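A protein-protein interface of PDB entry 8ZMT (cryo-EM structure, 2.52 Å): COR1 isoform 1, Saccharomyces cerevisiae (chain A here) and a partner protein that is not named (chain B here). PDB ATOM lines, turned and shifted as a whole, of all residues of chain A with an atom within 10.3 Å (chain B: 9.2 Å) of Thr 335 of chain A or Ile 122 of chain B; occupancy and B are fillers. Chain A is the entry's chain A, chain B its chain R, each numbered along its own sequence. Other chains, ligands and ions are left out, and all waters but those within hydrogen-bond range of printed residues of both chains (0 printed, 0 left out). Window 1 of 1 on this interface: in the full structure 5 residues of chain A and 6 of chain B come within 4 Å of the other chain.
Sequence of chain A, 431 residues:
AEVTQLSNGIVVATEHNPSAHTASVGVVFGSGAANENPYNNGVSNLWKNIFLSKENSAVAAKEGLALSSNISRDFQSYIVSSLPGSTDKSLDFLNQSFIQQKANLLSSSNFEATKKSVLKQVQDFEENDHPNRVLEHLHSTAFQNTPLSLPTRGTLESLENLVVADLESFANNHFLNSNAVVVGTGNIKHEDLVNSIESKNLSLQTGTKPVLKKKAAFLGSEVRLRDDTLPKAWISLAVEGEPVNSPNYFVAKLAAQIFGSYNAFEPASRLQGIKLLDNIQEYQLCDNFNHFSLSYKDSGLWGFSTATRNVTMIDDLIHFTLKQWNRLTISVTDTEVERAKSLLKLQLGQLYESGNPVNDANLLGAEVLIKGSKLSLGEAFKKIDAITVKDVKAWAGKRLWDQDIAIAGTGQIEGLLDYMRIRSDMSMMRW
NZ of Lys 275 of chain A lies within hydrogen-bond range of O of Asp 120 of chain B. The side-chain hydroxyl (OG1) of Thr 335 of chain A is in hydrogen-bond range of the backbone carbonyl oxygen (O) of Ile 122 of chain B. The side-chain amino group (NZ) of Lys 126 of chain B is in salt-bridge range of the side-chain carboxylate (OE2) of Glu 338 of chain A (3.7 Å).
The side-chain amino group (NZ) of Lys 341 of chain A is in salt-bridge range of the side-chain carboxylate (OE2) of Glu 338 of chain A. The side-chain amino group of Lys 116 of chain B is in salt-bridge range of the side-chain carboxylate of Asp 120 of chain B, 3.1 Å away.
Among the printed residues, pairs that only touch across the chains: Thr 335 of chain A with Val 124 of chain B (3.7 Å), Thr 335 of chain A with Glu 123 of chain B (3.8 Å), Glu 338 of chain A with Val 124 of chain B (3.9 Å) and Asp 334 of chain A with Val 124 of chain B (3.96 Å).
Of the printed residues of chain B, Asp 334 of chain A touches Val 124 (3.96 Å). Of the printed residues of chain B, Glu 338 of chain A touches Val 124 and Lys 126. No residue of chain A comes within 4 Å of Asn 121 of chain B. Ile 122 of chain B touches just one residue of chain A: Thr 335 (2.8 Å). Of the printed residues of chain A, Val 124 of chain B touches Asp 334, Thr 335 and Glu 338. Of the printed residues of chain A, Lys 126 of chain B touches Glu 338 (3.4 Å). The nearest residue of chain B that does not touch Thr 335 of chain A is Leu 119 of chain B (5.9 Å). The nearest residue of chain A that does not touch Ile 122 of chain B is Thr 333 of chain A (6.0 Å).
Of the 12 printed residues of chain B, 5 touch a printed residue of chain A. Of the 22 printed residues of chain A, 4 touch a printed residue of chain B.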
ATOM      1  N   LEU A 254     -29.828 -10.338  -2.069  1.00  0.00           N
ATOM      2  CA  LEU A 254     -29.773 -10.321  -0.613  1.00  0.00           C
ATOM      3  C   LEU A 254     -29.905  -8.903  -0.074  1.00  0.00           C
ATOM      4  O   LEU A 254     -30.390  -8.705   1.043  1.00  0.00           O
ATOM      5  CB  LEU A 254     -28.477 -10.982  -0.140  1.00  0.00           C
ATOM      6  CG  LEU A 254     -28.241 -11.271   1.344  1.00  0.00           C
ATOM      7  CD1 LEU A 254     -27.518 -12.575   1.487  1.00  0.00           C
ATOM      8  CD2 LEU A 254     -27.409 -10.189   1.993  1.00  0.00           C
ATOM      9  N   GLN A 257     -33.552  -8.045   0.196  1.00  0.00           N
ATOM     10  CA  GLN A 257     -34.200  -8.773   1.280  1.00  0.00           C
ATOM     11  C   GLN A 257     -33.932  -8.138   2.641  1.00  0.00           C
ATOM     12  O   GLN A 257     -34.660  -8.419   3.597  1.00  0.00           O
ATOM     13  CB  GLN A 257     -33.733 -10.233   1.245  1.00  0.00           C
ATOM     14  CG  GLN A 257     -34.545 -11.233   2.057  1.00  0.00           C
ATOM     15  CD  GLN A 257     -35.981 -11.350   1.606  1.00  0.00           C
ATOM     16  OE1 GLN A 257     -36.902 -11.075   2.368  1.00  0.00           O
ATOM     17  NE2 GLN A 257     -36.181 -11.772   0.369  1.00  0.00           N
ATOM     18  N   ILE A 258     -32.919  -7.273   2.746  1.00  0.00           N
ATOM     19  CA  ILE A 258     -32.642  -6.570   3.996  1.00  0.00           C
ATOM     20  C   ILE A 258     -33.758  -5.582   4.316  1.00  0.00           C
ATOM     21  O   ILE A 258     -34.173  -5.455   5.473  1.00  0.00           O
ATOM     22  CB  ILE A 258     -31.255  -5.891   3.909  1.00  0.00           C
ATOM     23  CG1 ILE A 258     -30.151  -6.945   3.964  1.00  0.00           C
ATOM     24  CG2 ILE A 258     -31.034  -4.887   5.024  1.00  0.00           C
ATOM     25  CD1 ILE A 258     -28.767  -6.399   3.760  1.00  0.00           C
ATOM     26  N   GLY A 273     -37.861  -7.327  11.721  1.00  0.00           N
ATOM     27  CA  GLY A 273     -36.582  -6.761  12.093  1.00  0.00           C
ATOM     28  C   GLY A 273     -35.980  -5.860  11.039  1.00  0.00           C
ATOM     29  O   GLY A 273     -34.907  -6.147  10.507  1.00  0.00           O
ATOM     30  N   ILE A 274     -36.665  -4.765  10.730  1.00  0.00           N
ATOM     31  CA  ILE A 274     -36.243  -3.800   9.723  1.00  0.00           C
ATOM     32  C   ILE A 274     -36.191  -2.434  10.387  1.00  0.00           C
ATOM     33  O   ILE A 274     -37.185  -1.987  10.967  1.00  0.00           O
ATOM     34  CB  ILE A 274     -37.201  -3.783   8.514  1.00  0.00           C
ATOM     35  CG1 ILE A 274     -37.269  -5.160   7.860  1.00  0.00           C
ATOM     36  CG2 ILE A 274     -36.775  -2.750   7.498  1.00  0.00           C
ATOM     37  CD1 ILE A 274     -38.505  -5.384   7.048  1.00  0.00           C
ATOM     38  N   LYS A 275     -35.038  -1.770  10.302  1.00  0.00           N
ATOM     39  CA  LYS A 275     -34.847  -0.480  10.954  1.00  0.00           C
ATOM     40  C   LYS A 275     -35.596   0.660  10.280  1.00  0.00           C
ATOM     41  O   LYS A 275     -35.727   1.728  10.882  1.00  0.00           O
ATOM     42  CB  LYS A 275     -33.361  -0.133  11.016  1.00  0.00           C
ATOM     43  CG  LYS A 275     -32.545  -1.064  11.875  1.00  0.00           C
ATOM     44  CD  LYS A 275     -31.116  -0.580  11.990  1.00  0.00           C
ATOM     45  CE  LYS A 275     -30.247  -1.592  12.714  1.00  0.00           C
ATOM     46  NZ  LYS A 275     -30.723  -1.842  14.097  1.00  0.00           N
ATOM     47  N   ARG A 327     -26.702   3.211   4.389  1.00  0.00           N
ATOM     48  CA  ARG A 327     -26.041   2.408   5.405  1.00  0.00           C
ATOM     49  C   ARG A 327     -25.429   1.129   4.857  1.00  0.00           C
ATOM     50  O   ARG A 327     -24.612   0.514   5.545  1.00  0.00           O
ATOM     51  CB  ARG A 327     -27.026   2.057   6.513  1.00  0.00           C
ATOM     52  CG  ARG A 327     -27.532   3.241   7.301  1.00  0.00           C
ATOM     53  CD  ARG A 327     -28.531   2.810   8.354  1.00  0.00           C
ATOM     54  NE  ARG A 327     -27.967   1.832   9.276  1.00  0.00           N
ATOM     55  CZ  ARG A 327     -28.366   0.570   9.364  1.00  0.00           C
ATOM     56  NH1 ARG A 327     -27.791  -0.248  10.230  1.00  0.00           N
ATOM     57  NH2 ARG A 327     -29.330   0.124   8.578  1.00  0.00           N
ATOM     58  N   SER A 331     -22.279   1.369   7.194  1.00  0.00           N
ATOM     59  CA  SER A 331     -22.544   0.861   8.540  1.00  0.00           C
ATOM     60  C   SER A 331     -23.595  -0.241   8.562  1.00  0.00           C
ATOM     61  O   SER A 331     -24.485  -0.242   9.415  1.00  0.00           O
ATOM     62  CB  SER A 331     -22.961   1.994   9.474  1.00  0.00           C
ATOM     63  OG  SER A 331     -24.215   2.527   9.105  1.00  0.00           O
ATOM     64  N   VAL A 332     -23.516  -1.203   7.653  1.00  0.00           N
ATOM     65  CA  VAL A 332     -24.411  -2.355   7.724  1.00  0.00           C
ATOM     66  C   VAL A 332     -23.835  -3.363   8.715  1.00  0.00           C
ATOM     67  O   VAL A 332     -22.617  -3.559   8.794  1.00  0.00           O
ATOM     68  CB  VAL A 332     -24.647  -2.950   6.317  1.00  0.00           C
ATOM     69  CG1 VAL A 332     -23.359  -3.428   5.661  1.00  0.00           C
ATOM     70  CG2 VAL A 332     -25.697  -4.052   6.341  1.00  0.00           C
ATOM     71  N   THR A 333     -24.702  -3.963   9.531  1.00  0.00           N
ATOM     72  CA  THR A 333     -24.258  -4.804  10.629  1.00  0.00           C
ATOM     73  C   THR A 333     -24.269  -6.277  10.229  1.00  0.00           C
ATOM     74  O   THR A 333     -24.569  -6.640   9.091  1.00  0.00           O
ATOM     75  CB  THR A 333     -25.116  -4.573  11.874  1.00  0.00           C
ATOM     76  OG1 THR A 333     -26.360  -5.263  11.737  1.00  0.00           O
ATOM     77  CG2 THR A 333     -25.384  -3.100  12.078  1.00  0.00           C
ATOM     78  N   ASP A 334     -23.936  -7.138  11.186  1.00  0.00           N
ATOM     79  CA  ASP A 334     -23.808  -8.569  10.958  1.00  0.00           C
ATOM     80  C   ASP A 334     -25.115  -9.317  11.153  1.00  0.00           C
ATOM     81  O   ASP A 334     -25.316 -10.369  10.541  1.00  0.00           O
ATOM     82  CB  ASP A 334     -22.754  -9.146  11.903  1.00  0.00           C
ATOM     83  CG  ASP A 334     -21.956 -10.261  11.278  1.00  0.00           C
ATOM     84  OD1 ASP A 334     -22.510 -11.007  10.448  1.00  0.00           O
ATOM     85  OD2 ASP A 334     -20.763 -10.389  11.618  1.00  0.00           O
ATOM     86  N   THR A 335     -26.006  -8.804  12.000  1.00  0.00           N
ATOM     87  CA  THR A 335     -27.282  -9.470  12.223  1.00  0.00           C
ATOM     88  C   THR A 335     -28.220  -9.265  11.040  1.00  0.00           C
ATOM     89  O   THR A 335     -29.044 -10.136  10.740  1.00  0.00           O
ATOM     90  CB  THR A 335     -27.899  -8.952  13.522  1.00  0.00           C
ATOM     91  OG1 THR A 335     -26.923  -9.032  14.563  1.00  0.00           O
ATOM     92  CG2 THR A 335     -29.083  -9.796  13.944  1.00  0.00           C
ATOM     93  N   GLU A 336     -28.076  -8.144  10.331  1.00  0.00           N
ATOM     94  CA  GLU A 336     -28.924  -7.875   9.177  1.00  0.00           C
ATOM     95  C   GLU A 336     -28.561  -8.756   7.989  1.00  0.00           C
ATOM     96  O   GLU A 336     -29.431  -9.082   7.178  1.00  0.00           O
ATOM     97  CB  GLU A 336     -28.834  -6.399   8.802  1.00  0.00           C
ATOM     98  CG  GLU A 336     -29.215  -5.474   9.939  1.00  0.00           C
ATOM     99  CD  GLU A 336     -29.271  -4.018   9.535  1.00  0.00           C
ATOM    100  OE1 GLU A 336     -30.375  -3.525   9.233  1.00  0.00           O
ATOM    101  OE2 GLU A 336     -28.216  -3.357   9.532  1.00  0.00           O
ATOM    102  N   VAL A 337     -27.298  -9.158   7.876  1.00  0.00           N
ATOM    103  CA  VAL A 337     -26.886 -10.029   6.781  1.00  0.00           C
ATOM    104  C   VAL A 337     -27.286 -11.475   7.062  1.00  0.00           C
ATOM    105  O   VAL A 337     -27.675 -12.210   6.151  1.00  0.00           O
ATOM    106  CB  VAL A 337     -25.371  -9.872   6.538  1.00  0.00           C
ATOM    107  CG1 VAL A 337     -24.889 -10.734   5.387  1.00  0.00           C
ATOM    108  CG2 VAL A 337     -25.045  -8.424   6.256  1.00  0.00           C
ATOM    109  N   GLU A 338     -27.236 -11.897   8.327  1.00  0.00           N
ATOM    110  CA  GLU A 338     -27.614 -13.265   8.666  1.00  0.00           C
ATOM    111  C   GLU A 338     -29.122 -13.465   8.637  1.00  0.00           C
ATOM    112  O   GLU A 338     -29.590 -14.577   8.378  1.00  0.00           O
ATOM    113  CB  GLU A 338     -27.065 -13.643  10.038  1.00  0.00           C
ATOM    114  CG  GLU A 338     -25.558 -13.671  10.108  1.00  0.00           C
ATOM    115  CD  GLU A 338     -24.936 -14.534   9.031  1.00  0.00           C
ATOM    116  OE1 GLU A 338     -25.314 -15.717   8.920  1.00  0.00           O
ATOM    117  OE2 GLU A 338     -24.063 -14.028   8.296  1.00  0.00           O
ATOM    118  N   ARG A 339     -29.893 -12.416   8.919  1.00  0.00           N
ATOM    119  CA  ARG A 339     -31.343 -12.516   8.819  1.00  0.00           C
ATOM    120  C   ARG A 339     -31.788 -12.585   7.364  1.00  0.00           C
ATOM    121  O   ARG A 339     -32.708 -13.335   7.024  1.00  0.00           O
ATOM    122  CB  ARG A 339     -31.993 -11.332   9.529  1.00  0.00           C
ATOM    123  CG  ARG A 339     -33.502 -11.283   9.454  1.00  0.00           C
ATOM    124  CD  ARG A 339     -34.001  -9.882   9.707  1.00  0.00           C
ATOM    125  NE  ARG A 339     -35.404  -9.720   9.352  1.00  0.00           N
ATOM    126  CZ  ARG A 339     -35.831  -9.210   8.203  1.00  0.00           C
ATOM    127  NH1 ARG A 339     -37.127  -9.102   7.970  1.00  0.00           N
ATOM    128  NH2 ARG A 339     -34.966  -8.811   7.288  1.00  0.00           N
ATOM    129  N   ALA A 340     -31.128 -11.827   6.489  1.00  0.00           N
ATOM    130  CA  ALA A 340     -31.511 -11.799   5.083  1.00  0.00           C
ATOM    131  C   ALA A 340     -31.049 -13.043   4.340  1.00  0.00           C
ATOM    132  O   ALA A 340     -31.553 -13.327   3.251  1.00  0.00           O
ATOM    133  CB  ALA A 340     -30.953 -10.551   4.415  1.00  0.00           C
ATOM    134  N   LYS A 341     -30.086 -13.783   4.891  1.00  0.00           N
ATOM    135  CA  LYS A 341     -29.688 -15.050   4.289  1.00  0.00           C
ATOM    136  C   LYS A 341     -30.779 -16.095   4.455  1.00  0.00           C
ATOM    137  O   LYS A 341     -31.052 -16.876   3.540  1.00  0.00           O
ATOM    138  CB  LYS A 341     -28.398 -15.553   4.925  1.00  0.00           C
ATOM    139  CG  LYS A 341     -27.131 -15.031   4.322  1.00  0.00           C
ATOM    140  CD  LYS A 341     -25.962 -15.704   4.980  1.00  0.00           C
ATOM    141  CE  LYS A 341     -24.675 -15.005   4.667  1.00  0.00           C
ATOM    142  NZ  LYS A 341     -23.518 -15.698   5.281  1.00  0.00           N
ATOM    143  N   SER A 342     -31.404 -16.129   5.629  1.00  0.00           N
ATOM    144  CA  SER A 342     -32.403 -17.147   5.916  1.00  0.00           C
ATOM    145  C   SER A 342     -33.715 -16.853   5.207  1.00  0.00           C
ATOM    146  O   SER A 342     -34.428 -17.777   4.805  1.00  0.00           O
ATOM    147  CB  SER A 342     -32.618 -17.242   7.421  1.00  0.00           C
ATOM    148  OG  SER A 342     -31.575 -17.967   8.029  1.00  0.00           O
ATOM    149  N   LEU A 343     -34.049 -15.574   5.045  1.00  0.00           N
ATOM    150  CA  LEU A 343     -35.302 -15.223   4.394  1.00  0.00           C
ATOM    151  C   LEU A 343     -35.195 -15.294   2.878  1.00  0.00           C
ATOM    152  O   LEU A 343     -36.216 -15.426   2.198  1.00  0.00           O
ATOM    153  CB  LEU A 343     -35.750 -13.834   4.837  1.00  0.00           C
ATOM    154  CG  LEU A 343     -36.296 -13.731   6.262  1.00  0.00           C
ATOM    155  CD1 LEU A 343     -36.690 -12.312   6.581  1.00  0.00           C
ATOM    156  CD2 LEU A 343     -37.468 -14.669   6.466  1.00  0.00           C
ATOM    157  N   THR A 388     -20.475 -12.175   2.662  1.00  0.00           N
ATOM    158  CA  THR A 388     -20.040 -11.519   3.885  1.00  0.00           C
ATOM    159  C   THR A 388     -20.507 -10.067   3.891  1.00  0.00           C
ATOM    160  O   THR A 388     -21.153  -9.592   2.959  1.00  0.00           O
ATOM    161  CB  THR A 388     -18.519 -11.602   4.031  1.00  0.00           C
ATOM    162  OG1 THR A 388     -17.896 -10.869   2.975  1.00  0.00           O
ATOM    163  CG2 THR A 388     -18.059 -13.040   3.961  1.00  0.00           C
ATOM    164  N   VAL A 389     -20.174  -9.359   4.972  1.00  0.00           N
ATOM    165  CA  VAL A 389     -20.493  -7.939   5.078  1.00  0.00           C
ATOM    166  C   VAL A 389     -19.623  -7.121   4.130  1.00  0.00           C
ATOM    167  O   VAL A 389     -20.046  -6.074   3.628  1.00  0.00           O
ATOM    168  CB  VAL A 389     -20.343  -7.488   6.548  1.00  0.00           C
ATOM    169  CG1 VAL A 389     -20.830  -6.069   6.758  1.00  0.00           C
ATOM    170  CG2 VAL A 389     -21.100  -8.427   7.455  1.00  0.00           C
ATOM    171  N   GLU B 115     -37.200  -5.312  26.038  1.00  0.00           N
ATOM    172  CA  GLU B 115     -37.061  -6.444  25.130  1.00  0.00           C
ATOM    173  C   GLU B 115     -36.917  -5.995  23.683  1.00  0.00           C
ATOM    174  O   GLU B 115     -36.288  -6.687  22.878  1.00  0.00           O
ATOM    175  CB  GLU B 115     -38.263  -7.373  25.284  1.00  0.00           C
ATOM    176  CG  GLU B 115     -38.056  -8.767  24.746  1.00  0.00           C
ATOM    177  CD  GLU B 115     -39.355  -9.432  24.361  1.00  0.00           C
ATOM    178  OE1 GLU B 115     -40.304  -8.712  23.993  1.00  0.00           O
ATOM    179  OE2 GLU B 115     -39.433 -10.674  24.431  1.00  0.00           O
ATOM    180  N   LYS B 116     -37.479  -4.840  23.335  1.00  0.00           N
ATOM    181  CA  LYS B 116     -37.309  -4.315  21.987  1.00  0.00           C
ATOM    182  C   LYS B 116     -35.920  -3.732  21.781  1.00  0.00           C
ATOM    183  O   LYS B 116     -35.440  -3.675  20.645  1.00  0.00           O
ATOM    184  CB  LYS B 116     -38.375  -3.262  21.705  1.00  0.00           C
ATOM    185  CG  LYS B 116     -38.695  -3.083  20.246  1.00  0.00           C
ATOM    186  CD  LYS B 116     -39.641  -1.930  20.040  1.00  0.00           C
ATOM    187  CE  LYS B 116     -39.858  -1.664  18.569  1.00  0.00           C
ATOM    188  NZ  LYS B 116     -38.571  -1.431  17.863  1.00  0.00           N
ATOM    189  N   ASP B 117     -35.260  -3.294  22.853  1.00  0.00           N
ATOM    190  CA  ASP B 117     -33.912  -2.751  22.730  1.00  0.00           C
ATOM    191  C   ASP B 117     -32.864  -3.849  22.622  1.00  0.00           C
ATOM    192  O   ASP B 117     -31.864  -3.685  21.920  1.00  0.00           O
ATOM    193  CB  ASP B 117     -33.592  -1.847  23.916  1.00  0.00           C
ATOM    194  CG  ASP B 117     -34.331  -0.539  23.860  1.00  0.00           C
ATOM    195  OD1 ASP B 117     -34.643  -0.084  22.741  1.00  0.00           O
ATOM    196  OD2 ASP B 117     -34.590   0.044  24.932  1.00  0.00           O
ATOM    197  N   GLU B 118     -33.067  -4.968  23.313  1.00  0.00           N
ATOM    198  CA  GLU B 118     -32.112  -6.063  23.241  1.00  0.00           C
ATOM    199  C   GLU B 118     -32.203  -6.830  21.931  1.00  0.00           C
ATOM    200  O   GLU B 118     -31.237  -7.494  21.554  1.00  0.00           O
ATOM    201  CB  GLU B 118     -32.318  -7.013  24.417  1.00  0.00           C
ATOM    202  CG  GLU B 118     -32.218  -6.334  25.764  1.00  0.00           C
ATOM    203  CD  GLU B 118     -32.633  -7.237  26.904  1.00  0.00           C
ATOM    204  OE1 GLU B 118     -31.812  -7.461  27.817  1.00  0.00           O
ATOM    205  OE2 GLU B 118     -33.783  -7.725  26.889  1.00  0.00           O
ATOM    206  N   LEU B 119     -33.334  -6.754  21.232  1.00  0.00           N
ATOM    207  CA  LEU B 119     -33.476  -7.406  19.940  1.00  0.00           C
ATOM    208  C   LEU B 119     -33.032  -6.528  18.781  1.00  0.00           C
ATOM    209  O   LEU B 119     -32.680  -7.056  17.723  1.00  0.00           O
ATOM    210  CB  LEU B 119     -34.928  -7.838  19.717  1.00  0.00           C
ATOM    211  CG  LEU B 119     -35.456  -8.988  20.575  1.00  0.00           C
ATOM    212  CD1 LEU B 119     -36.918  -9.240  20.291  1.00  0.00           C
ATOM    213  CD2 LEU B 119     -34.648 -10.238  20.340  1.00  0.00           C
ATOM    214  N   ASP B 120     -33.029  -5.211  18.952  1.00  0.00           N
ATOM    215  CA  ASP B 120     -32.577  -4.295  17.915  1.00  0.00           C
ATOM    216  C   ASP B 120     -31.079  -4.031  17.965  1.00  0.00           C
ATOM    217  O   ASP B 120     -30.551  -3.378  17.062  1.00  0.00           O
ATOM    218  CB  ASP B 120     -33.324  -2.962  18.013  1.00  0.00           C
ATOM    219  CG  ASP B 120     -34.775  -3.071  17.589  1.00  0.00           C
ATOM    220  OD1 ASP B 120     -35.090  -3.953  16.770  1.00  0.00           O
ATOM    221  OD2 ASP B 120     -35.597  -2.262  18.059  1.00  0.00           O
ATOM    222  N   ASN B 121     -30.387  -4.512  18.993  1.00  0.00           N
ATOM    223  CA  ASN B 121     -28.947  -4.348  19.145  1.00  0.00           C
ATOM    224  C   ASN B 121     -28.296  -5.683  19.468  1.00  0.00           C
ATOM    225  O   ASN B 121     -27.394  -5.771  20.301  1.00  0.00           O
ATOM    226  CB  ASN B 121     -28.627  -3.321  20.227  1.00  0.00           C
ATOM    227  CG  ASN B 121     -29.227  -1.962  19.941  1.00  0.00           C
ATOM    228  OD1 ASN B 121     -29.172  -1.470  18.817  1.00  0.00           O
ATOM    229  ND2 ASN B 121     -29.802  -1.345  20.962  1.00  0.00           N
ATOM    230  N   ILE B 122     -28.746  -6.742  18.807  1.00  0.00           N
ATOM    231  CA  ILE B 122     -28.326  -8.104  19.106  1.00  0.00           C
ATOM    232  C   ILE B 122     -27.182  -8.480  18.172  1.00  0.00           C
ATOM    233  O   ILE B 122     -27.030  -7.920  17.078  1.00  0.00           O
ATOM    234  CB  ILE B 122     -29.534  -9.069  18.994  1.00  0.00           C
ATOM    235  CG1 ILE B 122     -29.271 -10.412  19.684  1.00  0.00           C
ATOM    236  CG2 ILE B 122     -29.951  -9.276  17.551  1.00  0.00           C
ATOM    237  CD1 ILE B 122     -29.489 -10.390  21.170  1.00  0.00           C
ATOM    238  N   GLU B 123     -26.328  -9.393  18.630  1.00  0.00           N
ATOM    239  CA  GLU B 123     -25.200  -9.885  17.854  1.00  0.00           C
ATOM    240  C   GLU B 123     -25.398 -11.358  17.532  1.00  0.00           C
ATOM    241  O   GLU B 123     -25.848 -12.127  18.385  1.00  0.00           O
ATOM    242  CB  GLU B 123     -23.879  -9.699  18.612  1.00  0.00           C
ATOM    243  CG  GLU B 123     -23.290  -8.301  18.559  1.00  0.00           C
ATOM    244  CD  GLU B 123     -23.734  -7.429  19.711  1.00  0.00           C
ATOM    245  OE1 GLU B 123     -22.865  -6.816  20.364  1.00  0.00           O
ATOM    246  OE2 GLU B 123     -24.948  -7.357  19.979  1.00  0.00           O
ATOM    247  N   VAL B 124     -25.054 -11.750  16.302  1.00  0.00           N
ATOM    248  CA  VAL B 124     -25.138 -13.159  15.935  1.00  0.00           C
ATOM    249  C   VAL B 124     -23.971 -13.928  16.548  1.00  0.00           C
ATOM    250  O   VAL B 124     -22.900 -13.381  16.831  1.00  0.00           O
ATOM    251  CB  VAL B 124     -25.175 -13.337  14.408  1.00  0.00           C
ATOM    252  CG1 VAL B 124     -26.530 -12.916  13.857  1.00  0.00           C
ATOM    253  CG2 VAL B 124     -24.059 -12.544  13.750  1.00  0.00           C
ATOM    254  N   SER B 125     -24.188 -15.224  16.748  1.00  0.00           N
ATOM    255  CA  SER B 125     -23.264 -16.087  17.476  1.00  0.00           C
ATOM    256  C   SER B 125     -22.974 -17.355  16.682  1.00  0.00           C
ATOM    257  O   SER B 125     -23.103 -18.475  17.182  1.00  0.00           O
ATOM    258  CB  SER B 125     -23.814 -16.424  18.857  1.00  0.00           C
ATOM    259  OG  SER B 125     -24.996 -17.196  18.763  1.00  0.00           O
ATOM    260  N   LYS B 126     -22.597 -17.181  15.416  1.00  0.00           N
ATOM    261  CA  LYS B 126     -22.264 -18.289  14.516  1.00  0.00           C
ATOM    262  C   LYS B 126     -21.061 -19.100  14.998  1.00  0.00           C
ATOM    263  O   LYS B 126     -20.200 -18.595  15.722  1.00  0.00           O
ATOM    264  CB  LYS B 126     -21.986 -17.758  13.106  1.00  0.00           C
ATOM    265  CG  LYS B 126     -22.981 -16.720  12.615  1.00  0.00           C
ATOM    266  CD  LYS B 126     -22.822 -16.476  11.124  1.00  0.00           C
ATOM    267  CE  LYS B 126     -21.454 -15.898  10.791  1.00  0.00           C
ATOM    268  NZ  LYS B 126     -21.142 -16.015   9.340  1.00  0.00           N
ATOM    269  OXT LYS B 126     -20.930 -20.281  14.675  1.00  0.00           O
